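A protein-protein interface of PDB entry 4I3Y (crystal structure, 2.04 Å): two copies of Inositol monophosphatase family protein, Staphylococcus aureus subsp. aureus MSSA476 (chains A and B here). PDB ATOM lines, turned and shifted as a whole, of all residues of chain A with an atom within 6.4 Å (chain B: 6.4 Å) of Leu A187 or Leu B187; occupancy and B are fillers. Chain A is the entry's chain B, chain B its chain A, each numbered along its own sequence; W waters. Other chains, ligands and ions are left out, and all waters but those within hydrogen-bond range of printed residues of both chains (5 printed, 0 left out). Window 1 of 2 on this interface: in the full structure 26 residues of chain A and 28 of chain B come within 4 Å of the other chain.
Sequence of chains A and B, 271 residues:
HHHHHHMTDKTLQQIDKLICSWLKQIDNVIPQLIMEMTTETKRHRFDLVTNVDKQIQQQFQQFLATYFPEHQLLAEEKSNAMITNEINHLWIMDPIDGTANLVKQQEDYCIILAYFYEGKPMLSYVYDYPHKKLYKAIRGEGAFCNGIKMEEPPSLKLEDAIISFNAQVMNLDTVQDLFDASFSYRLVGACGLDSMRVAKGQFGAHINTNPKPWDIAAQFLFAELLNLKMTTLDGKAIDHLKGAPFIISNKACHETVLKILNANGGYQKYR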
ATOM      1  N   ILE A 163      17.295 -16.985 -10.880  1.00  0.00           N
ATOM      2  CA  ILE A 163      16.830 -15.581 -10.716  1.00  0.00           C
ATOM      3  C   ILE A 163      17.870 -14.777 -10.037  1.00  0.00           C
ATOM      4  O   ILE A 163      18.753 -15.336  -9.356  1.00  0.00           O
ATOM      5  CB  ILE A 163      15.517 -15.454  -9.914  1.00  0.00           C
ATOM      6  CG1 ILE A 163      15.715 -16.133  -8.553  1.00  0.00           C
ATOM      7  CG2 ILE A 163      14.413 -16.017 -10.812  1.00  0.00           C
ATOM      8  CD1 ILE A 163      14.808 -15.605  -7.525  1.00  0.00           C
ATOM      9  N   SER A 164      17.753 -13.481 -10.248  1.00  0.00           N
ATOM     10  CA  SER A 164      18.758 -12.541  -9.820  1.00  0.00           C
ATOM     11  C   SER A 164      18.089 -11.372  -9.103  1.00  0.00           C
ATOM     12  O   SER A 164      17.175 -10.725  -9.638  1.00  0.00           O
ATOM     13  CB  SER A 164      19.448 -12.018 -11.091  1.00  0.00           C
ATOM     14  OG  SER A 164      20.239 -10.896 -10.831  1.00  0.00           O
ATOM     15  N   PHE A 165      18.607 -11.032  -7.951  1.00  0.00           N
ATOM     16  CA  PHE A 165      18.108  -9.873  -7.268  1.00  0.00           C
ATOM     17  C   PHE A 165      19.143  -9.557  -6.154  1.00  0.00           C
ATOM     18  O   PHE A 165      20.111 -10.315  -5.906  1.00  0.00           O
ATOM     19  CB  PHE A 165      16.703 -10.145  -6.677  1.00  0.00           C
ATOM     20  CG  PHE A 165      16.644 -11.334  -5.750  1.00  0.00           C
ATOM     21  CD1 PHE A 165      16.894 -11.188  -4.383  1.00  0.00           C
ATOM     22  CD2 PHE A 165      16.292 -12.624  -6.244  1.00  0.00           C
ATOM     23  CE1 PHE A 165      16.803 -12.295  -3.511  1.00  0.00           C
ATOM     24  CE2 PHE A 165      16.231 -13.739  -5.380  1.00  0.00           C
ATOM     25  CZ  PHE A 165      16.455 -13.586  -4.027  1.00  0.00           C
ATOM     26  N   ASN A 166      18.936  -8.419  -5.518  1.00  0.00           N
ATOM     27  CA  ASN A 166      19.763  -8.012  -4.380  1.00  0.00           C
ATOM     28  C   ASN A 166      19.127  -8.559  -3.114  1.00  0.00           C
ATOM     29  O   ASN A 166      18.102  -8.029  -2.657  1.00  0.00           O
ATOM     30  CB  ASN A 166      19.865  -6.471  -4.282  1.00  0.00           C
ATOM     31  CG  ASN A 166      20.852  -6.037  -3.173  1.00  0.00           C
ATOM     32  OD1 ASN A 166      21.276  -6.874  -2.339  1.00  0.00           O
ATOM     33  ND2 ASN A 166      21.296  -4.785  -3.215  1.00  0.00           N
ATOM     34  N   ALA A 167      19.726  -9.572  -2.508  1.00  0.00           N
ATOM     35  CA  ALA A 167      19.124 -10.186  -1.313  1.00  0.00           C
ATOM     36  C   ALA A 167      19.248  -9.323  -0.049  1.00  0.00           C
ATOM     37  O   ALA A 167      18.477  -9.549   0.902  1.00  0.00           O
ATOM     38  CB  ALA A 167      19.711 -11.569  -1.041  1.00  0.00           C
ATOM     39  N   GLN A 168      20.163  -8.325  -0.066  1.00  0.00           N
ATOM     40  CA  GLN A 168      20.475  -7.500   1.143  1.00  0.00           C
ATOM     41  C   GLN A 168      19.426  -6.417   1.400  1.00  0.00           C
ATOM     42  O   GLN A 168      19.429  -5.800   2.493  1.00  0.00           O
ATOM     43  CB  GLN A 168      21.854  -6.834   0.997  1.00  0.00           C
ATOM     44  CG  GLN A 168      22.976  -7.781   0.435  1.00  0.00           C
ATOM     45  CD  GLN A 168      24.378  -7.131   0.332  1.00  0.00           C
ATOM     46  OE1 GLN A 168      24.996  -7.081  -0.766  1.00  0.00           O
ATOM     47  NE2 GLN A 168      24.850  -6.591   1.443  1.00  0.00           N
ATOM     48  N   SER A 184      17.617 -21.690  -9.151  1.00  0.00           N
ATOM     49  CA  SER A 184      18.735 -21.267  -8.338  1.00  0.00           C
ATOM     50  C   SER A 184      18.831 -19.729  -8.420  1.00  0.00           C
ATOM     51  O   SER A 184      17.994 -19.103  -9.033  1.00  0.00           O
ATOM     52  CB  SER A 184      20.020 -21.870  -8.855  1.00  0.00           C
ATOM     53  OG  SER A 184      21.097 -21.742  -7.942  1.00  0.00           O
ATOM     54  N   TYR A 185      19.911 -19.173  -7.864  1.00  0.00           N
ATOM     55  CA  TYR A 185      20.064 -17.748  -7.638  1.00  0.00           C
ATOM     56  C   TYR A 185      21.475 -17.329  -8.074  1.00  0.00           C
ATOM     57  O   TYR A 185      22.423 -17.985  -7.742  1.00  0.00           O
ATOM     58  CB  TYR A 185      19.819 -17.432  -6.127  1.00  0.00           C
ATOM     59  CG  TYR A 185      20.276 -16.041  -5.730  1.00  0.00           C
ATOM     60  CD1 TYR A 185      19.497 -14.898  -6.022  1.00  0.00           C
ATOM     61  CD2 TYR A 185      21.434 -15.857  -5.028  1.00  0.00           C
ATOM     62  CE1 TYR A 185      19.925 -13.621  -5.658  1.00  0.00           C
ATOM     63  CE2 TYR A 185      21.843 -14.567  -4.635  1.00  0.00           C
ATOM     64  CZ  TYR A 185      21.088 -13.443  -4.951  1.00  0.00           C
ATOM     65  OH  TYR A 185      21.506 -12.147  -4.555  1.00  0.00           O
ATOM     66  N   ARG A 186      21.604 -16.271  -8.857  1.00  0.00           N
ATOM     67  CA  ARG A 186      22.946 -15.735  -9.175  1.00  0.00           C
ATOM     68  C   ARG A 186      22.820 -14.235  -9.116  1.00  0.00           C
ATOM     69  O   ARG A 186      21.702 -13.712  -9.239  1.00  0.00           O
ATOM     70  CB  ARG A 186      23.373 -16.077 -10.631  1.00  0.00           C
ATOM     71  CG  ARG A 186      23.372 -17.540 -11.080  1.00  0.00           C
ATOM     72  CD  ARG A 186      24.655 -18.329 -10.955  1.00  0.00           C
ATOM     73  NE  ARG A 186      24.298 -19.114  -9.884  1.00  0.00           N
ATOM     74  CZ  ARG A 186      23.965 -20.409  -9.802  1.00  0.00           C
ATOM     75  NH1 ARG A 186      24.183 -21.378 -10.699  1.00  0.00           N
ATOM     76  NH2 ARG A 186      23.475 -20.704  -8.638  1.00  0.00           N
ATOM     77  N   LEU A 187      23.951 -13.553  -9.012  1.00  0.00           N
ATOM     78  CA  LEU A 187      23.965 -12.105  -9.148  1.00  0.00           C
ATOM     79  C   LEU A 187      25.204 -11.591  -9.862  1.00  0.00           C
ATOM     80  O   LEU A 187      26.346 -11.879  -9.420  1.00  0.00           O
ATOM     81  CB  LEU A 187      23.807 -11.417  -7.802  1.00  0.00           C
ATOM     82  CG  LEU A 187      23.872  -9.884  -7.826  1.00  0.00           C
ATOM     83  CD1 LEU A 187      22.638  -9.378  -8.584  1.00  0.00           C
ATOM     84  CD2 LEU A 187      23.723  -9.480  -6.368  1.00  0.00           C
ATOM     85  N   VAL A 188      24.968 -10.863 -10.971  1.00  0.00           N
ATOM     86  CA  VAL A 188      26.043 -10.187 -11.710  1.00  0.00           C
ATOM     87  C   VAL A 188      26.340  -8.853 -11.018  1.00  0.00           C
ATOM     88  O   VAL A 188      27.536  -8.518 -10.774  1.00  0.00           O
ATOM     89  CB  VAL A 188      25.720  -9.997 -13.213  1.00  0.00           C
ATOM     90  CG1 VAL A 188      26.779  -9.199 -13.969  1.00  0.00           C
ATOM     91  CG2 VAL A 188      25.500 -11.350 -13.897  1.00  0.00           C
ATOM     92  N   GLY A 189      25.287  -8.103 -10.679  1.00  0.00           N
ATOM     93  CA  GLY A 189      25.554  -6.901  -9.853  1.00  0.00           C
ATOM     94  C   GLY A 189      25.594  -5.598 -10.674  1.00  0.00           C
ATOM     95  O   GLY A 189      25.902  -4.494 -10.144  1.00  0.00           O
ATOM     96  N   ALA A 190      25.247  -5.687 -11.959  1.00  0.00           N
ATOM     97  CA  ALA A 190      24.925  -4.478 -12.705  1.00  0.00           C
ATOM     98  C   ALA A 190      23.524  -4.666 -13.300  1.00  0.00           C
ATOM     99  O   ALA A 190      23.321  -5.591 -14.073  1.00  0.00           O
ATOM    100  CB  ALA A 190      25.963  -4.263 -13.852  1.00  0.00           C
ATOM    101  N   ASP A 194      22.488  -7.972 -15.518  1.00  0.00           N
ATOM    102  CA  ASP A 194      21.493  -8.933 -14.944  1.00  0.00           C
ATOM    103  C   ASP A 194      20.284  -8.916 -15.849  1.00  0.00           C
ATOM    104  O   ASP A 194      19.779  -9.971 -16.194  1.00  0.00           O
ATOM    105  CB  ASP A 194      21.086  -8.594 -13.507  1.00  0.00           C
ATOM    106  CG  ASP A 194      22.162  -8.985 -12.483  1.00  0.00           C
ATOM    107  OD1 ASP A 194      22.388 -10.189 -12.259  1.00  0.00           O
ATOM    108  OD2 ASP A 194      22.828  -8.084 -11.946  1.00  0.00           O
ATOM    109  N   PHE A 203      18.699 -16.020 -17.394  1.00  0.00           N
ATOM    110  CA  PHE A 203      17.913 -15.847 -16.136  1.00  0.00           C
ATOM    111  C   PHE A 203      16.422 -15.829 -16.497  1.00  0.00           C
ATOM    112  O   PHE A 203      16.063 -15.372 -17.585  1.00  0.00           O
ATOM    113  CB  PHE A 203      18.252 -14.545 -15.387  1.00  0.00           C
ATOM    114  CG  PHE A 203      19.713 -14.456 -14.832  1.00  0.00           C
ATOM    115  CD1 PHE A 203      20.507 -15.570 -14.669  1.00  0.00           C
ATOM    116  CD2 PHE A 203      20.237 -13.218 -14.428  1.00  0.00           C
ATOM    117  CE1 PHE A 203      21.839 -15.477 -14.176  1.00  0.00           C
ATOM    118  CE2 PHE A 203      21.538 -13.110 -13.912  1.00  0.00           C
ATOM    119  CZ  PHE A 203      22.331 -14.236 -13.777  1.00  0.00           C
ATOM    120  N   HIS A 206      15.052 -10.637 -13.330  1.00  0.00           N
ATOM    121  CA  HIS A 206      15.907  -9.787 -12.497  1.00  0.00           C
ATOM    122  C   HIS A 206      15.004  -8.784 -11.775  1.00  0.00           C
ATOM    123  O   HIS A 206      14.085  -8.219 -12.404  1.00  0.00           O
ATOM    124  CB  HIS A 206      16.920  -9.012 -13.347  1.00  0.00           C
ATOM    125  CG  HIS A 206      17.740  -8.092 -12.525  1.00  0.00           C
ATOM    126  ND1 HIS A 206      18.517  -8.536 -11.465  1.00  0.00           N
ATOM    127  CD2 HIS A 206      17.874  -6.747 -12.561  1.00  0.00           C
ATOM    128  CE1 HIS A 206      19.148  -7.507 -10.930  1.00  0.00           C
ATOM    129  NE2 HIS A 206      18.747  -6.405 -11.544  1.00  0.00           N
ATOM    130  N   ASP B 108      29.561 -19.034 -17.668  1.00  0.00           N
ATOM    131  CA  ASP B 108      29.916 -19.183 -16.219  1.00  0.00           C
ATOM    132  C   ASP B 108      30.108 -20.632 -15.793  1.00  0.00           C
ATOM    133  O   ASP B 108      29.585 -21.078 -14.735  1.00  0.00           O
ATOM    134  CB  ASP B 108      28.923 -18.437 -15.294  1.00  0.00           C
ATOM    135  CG  ASP B 108      29.030 -16.928 -15.474  1.00  0.00           C
ATOM    136  OD1 ASP B 108      30.084 -16.493 -15.999  1.00  0.00           O
ATOM    137  OD2 ASP B 108      28.118 -16.178 -15.085  1.00  0.00           O
ATOM    138  N   ILE B 162      34.103  -7.716  -1.974  1.00  0.00           N
ATOM    139  CA  ILE B 162      32.899  -8.437  -2.373  1.00  0.00           C
ATOM    140  C   ILE B 162      33.046  -9.872  -1.916  1.00  0.00           C
ATOM    141  O   ILE B 162      34.101 -10.438  -2.051  1.00  0.00           O
ATOM    142  CB  ILE B 162      32.666  -8.375  -3.920  1.00  0.00           C
ATOM    143  CG1 ILE B 162      32.339  -6.926  -4.319  1.00  0.00           C
ATOM    144  CG2 ILE B 162      31.596  -9.370  -4.367  1.00  0.00           C
ATOM    145  CD1 ILE B 162      32.366  -6.694  -5.825  1.00  0.00           C
ATOM    146  N   ILE B 163      32.010 -10.467  -1.348  1.00  0.00           N
ATOM    147  CA  ILE B 163      32.150 -11.904  -1.079  1.00  0.00           C
ATOM    148  C   ILE B 163      31.141 -12.723  -1.796  1.00  0.00           C
ATOM    149  O   ILE B 163      30.108 -12.206  -2.236  1.00  0.00           O
ATOM    150  CB  ILE B 163      32.090 -12.301   0.399  1.00  0.00           C
ATOM    151  CG1 ILE B 163      30.823 -11.819   1.082  1.00  0.00           C
ATOM    152  CG2 ILE B 163      33.334 -11.824   1.117  1.00  0.00           C
ATOM    153  CD1 ILE B 163      30.846 -12.453   2.475  1.00  0.00           C
ATOM    154  N   SER B 164      31.440 -14.015  -1.889  1.00  0.00           N
ATOM    155  CA  SER B 164      30.660 -14.924  -2.685  1.00  0.00           C
ATOM    156  C   SER B 164      30.474 -16.243  -1.938  1.00  0.00           C
ATOM    157  O   SER B 164      31.428 -16.803  -1.327  1.00  0.00           O
ATOM    158  CB  SER B 164      31.446 -15.134  -3.989  1.00  0.00           C
ATOM    159  OG  SER B 164      31.221 -16.375  -4.600  1.00  0.00           O
ATOM    160  N   PHE B 165      29.250 -16.762  -1.979  1.00  0.00           N
ATOM    161  CA  PHE B 165      28.932 -18.012  -1.299  1.00  0.00           C
ATOM    162  C   PHE B 165      27.512 -18.354  -1.691  1.00  0.00           C
ATOM    163  O   PHE B 165      26.785 -17.481  -2.246  1.00  0.00           O
ATOM    164  CB  PHE B 165      29.067 -17.890   0.246  1.00  0.00           C
ATOM    165  CG  PHE B 165      28.187 -16.812   0.862  1.00  0.00           C
ATOM    166  CD1 PHE B 165      26.883 -17.102   1.283  1.00  0.00           C
ATOM    167  CD2 PHE B 165      28.676 -15.527   1.059  1.00  0.00           C
ATOM    168  CE1 PHE B 165      26.068 -16.118   1.845  1.00  0.00           C
ATOM    169  CE2 PHE B 165      27.869 -14.528   1.624  1.00  0.00           C
ATOM    170  CZ  PHE B 165      26.555 -14.824   1.987  1.00  0.00           C
ATOM    171  N   ASN B 166      27.136 -19.616  -1.444  1.00  0.00           N
ATOM    172  CA  ASN B 166      25.773 -20.105  -1.720  1.00  0.00           C
ATOM    173  C   ASN B 166      24.936 -19.767  -0.489  1.00  0.00           C
ATOM    174  O   ASN B 166      25.062 -20.388   0.579  1.00  0.00           O
ATOM    175  CB  ASN B 166      25.784 -21.608  -2.040  1.00  0.00           C
ATOM    176  CG  ASN B 166      24.387 -22.178  -2.302  1.00  0.00           C
ATOM    177  OD1 ASN B 166      23.378 -21.487  -2.210  1.00  0.00           O
ATOM    178  ND2 ASN B 166      24.336 -23.451  -2.644  1.00  0.00           N
ATOM    179  N   ALA B 167      24.104 -18.748  -0.639  1.00  0.00           N
ATOM    180  CA  ALA B 167      23.311 -18.231   0.492  1.00  0.00           C
ATOM    181  C   ALA B 167      22.089 -19.149   0.780  1.00  0.00           C
ATOM    182  O   ALA B 167      21.317 -18.896   1.733  1.00  0.00           O
ATOM    183  CB  ALA B 167      22.843 -16.825   0.173  1.00  0.00           C
ATOM    184  N   GLN B 168      21.882 -20.177  -0.044  1.00  0.00           N
ATOM    185  CA  GLN B 168      20.649 -20.993   0.068  1.00  0.00           C
ATOM    186  C   GLN B 168      20.892 -22.166   0.962  1.00  0.00           C
ATOM    187  O   GLN B 168      19.981 -22.885   1.297  1.00  0.00           O
ATOM    188  CB  GLN B 168      20.184 -21.555  -1.273  1.00  0.00           C
ATOM    189  CG  GLN B 168      20.106 -20.535  -2.372  1.00  0.00           C
ATOM    190  CD  GLN B 168      19.514 -21.090  -3.647  1.00  0.00           C
ATOM    191  OE1 GLN B 168      19.998 -20.824  -4.736  1.00  0.00           O
ATOM    192  NE2 GLN B 168      18.490 -21.883  -3.507  1.00  0.00           N
ATOM    193  N   SER B 184      29.997  -5.841  -0.547  1.00  0.00           N
ATOM    194  CA  SER B 184      28.767  -6.364  -1.252  1.00  0.00           C
ATOM    195  C   SER B 184      28.859  -7.889  -1.472  1.00  0.00           C
ATOM    196  O   SER B 184      29.851  -8.543  -1.106  1.00  0.00           O
ATOM    197  CB  SER B 184      28.524  -5.622  -2.569  1.00  0.00           C
ATOM    198  OG  SER B 184      27.187  -5.706  -3.069  1.00  0.00           O
ATOM    199  N   TYR B 185      27.820  -8.443  -2.072  1.00  0.00           N
ATOM    200  CA  TYR B 185      27.734  -9.878  -2.347  1.00  0.00           C
ATOM    201  C   TYR B 185      27.514 -10.097  -3.844  1.00  0.00           C
ATOM    202  O   TYR B 185      26.701  -9.395  -4.461  1.00  0.00           O
ATOM    203  CB  TYR B 185      26.529 -10.475  -1.597  1.00  0.00           C
ATOM    204  CG  TYR B 185      26.108 -11.860  -2.011  1.00  0.00           C
ATOM    205  CD1 TYR B 185      26.711 -12.971  -1.456  1.00  0.00           C
ATOM    206  CD2 TYR B 185      25.084 -12.060  -2.950  1.00  0.00           C
ATOM    207  CE1 TYR B 185      26.336 -14.252  -1.819  1.00  0.00           C
ATOM    208  CE2 TYR B 185      24.729 -13.359  -3.363  1.00  0.00           C
ATOM    209  CZ  TYR B 185      25.341 -14.460  -2.777  1.00  0.00           C
ATOM    210  OH  TYR B 185      24.963 -15.801  -3.083  1.00  0.00           O
ATOM    211  N   ARG B 186      28.165 -11.124  -4.382  1.00  0.00           N
ATOM    212  CA  ARG B 186      28.076 -11.462  -5.768  1.00  0.00           C
ATOM    213  C   ARG B 186      28.111 -13.013  -5.821  1.00  0.00           C
ATOM    214  O   ARG B 186      28.644 -13.680  -4.903  1.00  0.00           O
ATOM    215  CB  ARG B 186      29.188 -10.696  -6.611  1.00  0.00           C
ATOM    216  CG  ARG B 186      28.525  -9.680  -7.603  1.00  0.00           C
ATOM    217  CD  ARG B 186      28.984  -8.236  -7.775  1.00  0.00           C
ATOM    218  NE  ARG B 186      28.093  -7.655  -6.907  1.00  0.00           N
ATOM    219  CZ  ARG B 186      27.862  -6.428  -6.514  1.00  0.00           C
ATOM    220  NH1 ARG B 186      28.396  -5.308  -6.973  1.00  0.00           N
ATOM    221  NH2 ARG B 186      27.018  -6.419  -5.518  1.00  0.00           N
ATOM    222  N   LEU B 187      27.559 -13.603  -6.875  1.00  0.00           N
ATOM    223  CA  LEU B 187      27.783 -15.040  -7.096  1.00  0.00           C
ATOM    224  C   LEU B 187      27.878 -15.388  -8.542  1.00  0.00           C
ATOM    225  O   LEU B 187      26.896 -15.208  -9.306  1.00  0.00           O
ATOM    226  CB  LEU B 187      26.727 -15.891  -6.391  1.00  0.00           C
ATOM    227  CG  LEU B 187      26.781 -17.421  -6.557  1.00  0.00           C
ATOM    228  CD1 LEU B 187      28.023 -18.075  -5.917  1.00  0.00           C
ATOM    229  CD2 LEU B 187      25.580 -18.010  -5.867  1.00  0.00           C
ATOM    230  N   VAL B 188      29.015 -15.937  -8.946  1.00  0.00           N
ATOM    231  CA  VAL B 188      29.138 -16.499 -10.333  1.00  0.00           C
ATOM    232  C   VAL B 188      28.423 -17.888 -10.432  1.00  0.00           C
ATOM    233  O   VAL B 188      27.741 -18.186 -11.432  1.00  0.00           O
ATOM    234  CB  VAL B 188      30.630 -16.641 -10.753  1.00  0.00           C
ATOM    235  CG1 VAL B 188      30.745 -17.156 -12.166  1.00  0.00           C
ATOM    236  CG2 VAL B 188      31.390 -15.297 -10.617  1.00  0.00           C
ATOM    237  N   GLY B 189      28.639 -18.733  -9.421  1.00  0.00           N
ATOM    238  CA  GLY B 189      27.992 -20.025  -9.353  1.00  0.00           C
ATOM    239  C   GLY B 189      28.762 -21.234  -9.876  1.00  0.00           C
ATOM    240  O   GLY B 189      28.203 -22.351  -9.987  1.00  0.00           O
ATOM    241  N   ALA B 190      30.033 -21.024 -10.215  1.00  0.00           N
ATOM    242  CA  ALA B 190      30.965 -22.120 -10.424  1.00  0.00           C
ATOM    243  C   ALA B 190      32.097 -21.990  -9.414  1.00  0.00           C
ATOM    244  O   ALA B 190      32.785 -21.006  -9.407  1.00  0.00           O
ATOM    245  CB  ALA B 190      31.505 -22.074 -11.879  1.00  0.00           C
ATOM    246  N   ASP B 194      34.331 -18.586  -9.144  1.00  0.00           N
ATOM    247  CA  ASP B 194      34.242 -17.716  -7.990  1.00  0.00           C
ATOM    248  C   ASP B 194      35.622 -17.761  -7.285  1.00  0.00           C
ATOM    249  O   ASP B 194      36.063 -16.734  -6.709  1.00  0.00           O
ATOM    250  CB  ASP B 194      33.153 -18.200  -6.997  1.00  0.00           C
ATOM    251  CG  ASP B 194      31.725 -17.881  -7.443  1.00  0.00           C
ATOM    252  OD1 ASP B 194      31.250 -16.701  -7.274  1.00  0.00           O
ATOM    253  OD2 ASP B 194      31.048 -18.870  -7.883  1.00  0.00           O
ATOM    254  N   PHE B 203      37.064 -10.566  -5.722  1.00  0.00           N
ATOM    255  CA  PHE B 203      36.322 -10.933  -4.499  1.00  0.00           C
ATOM    256  C   PHE B 203      37.334 -11.054  -3.347  1.00  0.00           C
ATOM    257  O   PHE B 203      38.484 -11.434  -3.585  1.00  0.00           O
ATOM    258  CB  PHE B 203      35.663 -12.327  -4.697  1.00  0.00           C
ATOM    259  CG  PHE B 203      34.536 -12.355  -5.715  1.00  0.00           C
ATOM    260  CD1 PHE B 203      34.043 -11.191  -6.263  1.00  0.00           C
ATOM    261  CD2 PHE B 203      33.882 -13.568  -5.999  1.00  0.00           C
ATOM    262  CE1 PHE B 203      32.969 -11.233  -7.197  1.00  0.00           C
ATOM    263  CE2 PHE B 203      32.826 -13.630  -6.889  1.00  0.00           C
ATOM    264  CZ  PHE B 203      32.374 -12.453  -7.512  1.00  0.00           C
ATOM    265  N   HIS B 206      35.588 -16.620  -1.222  1.00  0.00           N
ATOM    266  CA  HIS B 206      34.556 -17.489  -1.737  1.00  0.00           C
ATOM    267  C   HIS B 206      34.437 -18.631  -0.750  1.00  0.00           C
ATOM    268  O   HIS B 206      35.447 -19.222  -0.297  1.00  0.00           O
ATOM    269  CB  HIS B 206      34.833 -18.071  -3.156  1.00  0.00           C
ATOM    270  CG  HIS B 206      33.823 -19.110  -3.581  1.00  0.00           C
ATOM    271  ND1 HIS B 206      32.490 -18.815  -3.769  1.00  0.00           N
ATOM    272  CD2 HIS B 206      33.958 -20.426  -3.901  1.00  0.00           C
ATOM    273  CE1 HIS B 206      31.834 -19.910  -4.118  1.00  0.00           C
ATOM    274  NE2 HIS B 206      32.701 -20.906  -4.200  1.00  0.00           N
HETATM  275  O   HOH W   1      26.431 -23.672 -11.736  1.00  0.00           O
HETATM  276  O   HOH W   2      24.459  -8.195  -3.600  1.00  0.00           O
HETATM  277  O   HOH W   3      22.771 -19.711  -5.288  1.00  0.00           O
HETATM  278  O   HOH W   4      27.724  -7.344   1.440  1.00  0.00           O
HETATM  279  O   HOH W   5      28.139  -2.897  -9.428  1.00  0.00           O
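The side-chain carboxylate (OD1) of Asp B194 lies within hydrogen-bond range of the backbone NH (N) of Val B188 (2.9 Å). The backbone NH of Gly B189 is in hydrogen-bond range of the side-chain carboxylate of Asp B194, at 2.9 Å. The backbone carbonyl oxygen (O) of Ser A184 sits at hydrogen-bond distance from the backbone NH (N) of Ile A163 (2.9 Å). The backbone carbonyl oxygen (O) of Ile A163 is in hydrogen-bond range of the backbone NH (N) of Arg A186 (3.0 Å). The side-chain amide oxygen of Asn A166 lies within hydrogen-bond range of the backbone NH of Gln A168 (2.9 Å). OG of Ser A184 lies within hydrogen-bond range of NH2 of Arg A186, 2.7 Å away.
Gln A168 touches Ser B184, and with the chains exchanged Ser A184 touches Gln B168. Tyr B185 touches its own counterpart, Tyr A185. Tyr A185 touches Leu B187, and with the chains exchanged Leu A187 touches Tyr B185. Leu A187 touches its own counterpart, Leu B187. Of the 14 pairs that touch across the chains among the printed residues, 14 have their exchanged pair printed and touching as well.
Ser A164 touches none of the printed residues of chain B. Printed residues of chain B within 4 Å of Ser A184: Gln B168. Leu A187 touches just these residues of chain B: Tyr B185, Arg B186 and Leu B187. Printed residues of chain B within 4 Å of Val A188: Arg B186 (3.3 Å). Of the printed residues of chain A, Ser B184 touches Gln A168. Leu B187 touches just these residues of chain A: Tyr A185 (3.7 Å), Arg A186 (3.9 Å) and Leu A187 (3.3 Å). Phe B203 touches none of the printed residues of chain A. The nearest residue of chain B that does not touch Leu A187 is Val B188 (4.9 Å). The nearest residue of chain A that does not touch Leu B187 is Val A188 (5.0 Å). The nearest printed residue of chain B that does not touch Ser A184 is Asn B166 (6.2 Å).
Ser A184 touches Gln B168. CE2 of Tyr B185 touches CE2 of Tyr A185, at 3.4 Å. Tyr A185 touches Leu B187. O of Leu B187 touches CB of Arg A186 (3.9 Å). Val B188 touches Arg A186. Arg A186 touches Gly B189. Tyr B185 touches Leu A187. O of Leu A187 touches CG of Arg B186, 3.6 Å away. Val A188 touches Arg B186. Arg B186 touches Gly A189 (NE to CA, 3.96 Å).
Of the 16 printed residues of chain A, 7 touch a printed residue of chain B. Hydrophobic or aromatic side chains of chain B within 4 Å of the printed part of chain A: Tyr B185 and Leu B187. Among the printed residues, 14 pairs touch across the chains. Among the printed residues, no Asp or Glu carboxylate lies within 4 Å of a Lys or Arg side-chain nitrogen of the other chain.
OE1 of Gln A168 is in hydrogen-bond range of OG of Ser B184. OE1 of Gln A168 lies within hydrogen-bond range of N of Tyr B185 (3.4 Å). O of Leu A187 sits at hydrogen-bond distance from N of Leu B187.
Water W2 lies within hydrogen-bond range of the backbone carbonyl oxygen of Tyr B185 (2.7 Å) and the side-chain amide oxygen of Gln A168 (3.1 Å). Water W1 bridges the backbone carbonyl oxygen (O) of Gly B189 (2.8 Å) and the guanidinium group (NH1) of Arg A186 (3.4 Å). Water W5 lies within hydrogen-bond range of O of Gly A189 (2.8 Å) and NH1 of Arg B186 (3.5 Å). Water W4 lies within hydrogen-bond range of the side-chain amide nitrogen of Gln A168 (3.0 Å) and the backbone NH of Ser B184 (3.4 Å). Water W3 bridges the backbone carbonyl oxygen (O) of Tyr A185 (3.0 Å) and the side-chain amide oxygen (OE1) of Gln B168 (3.0 Å).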
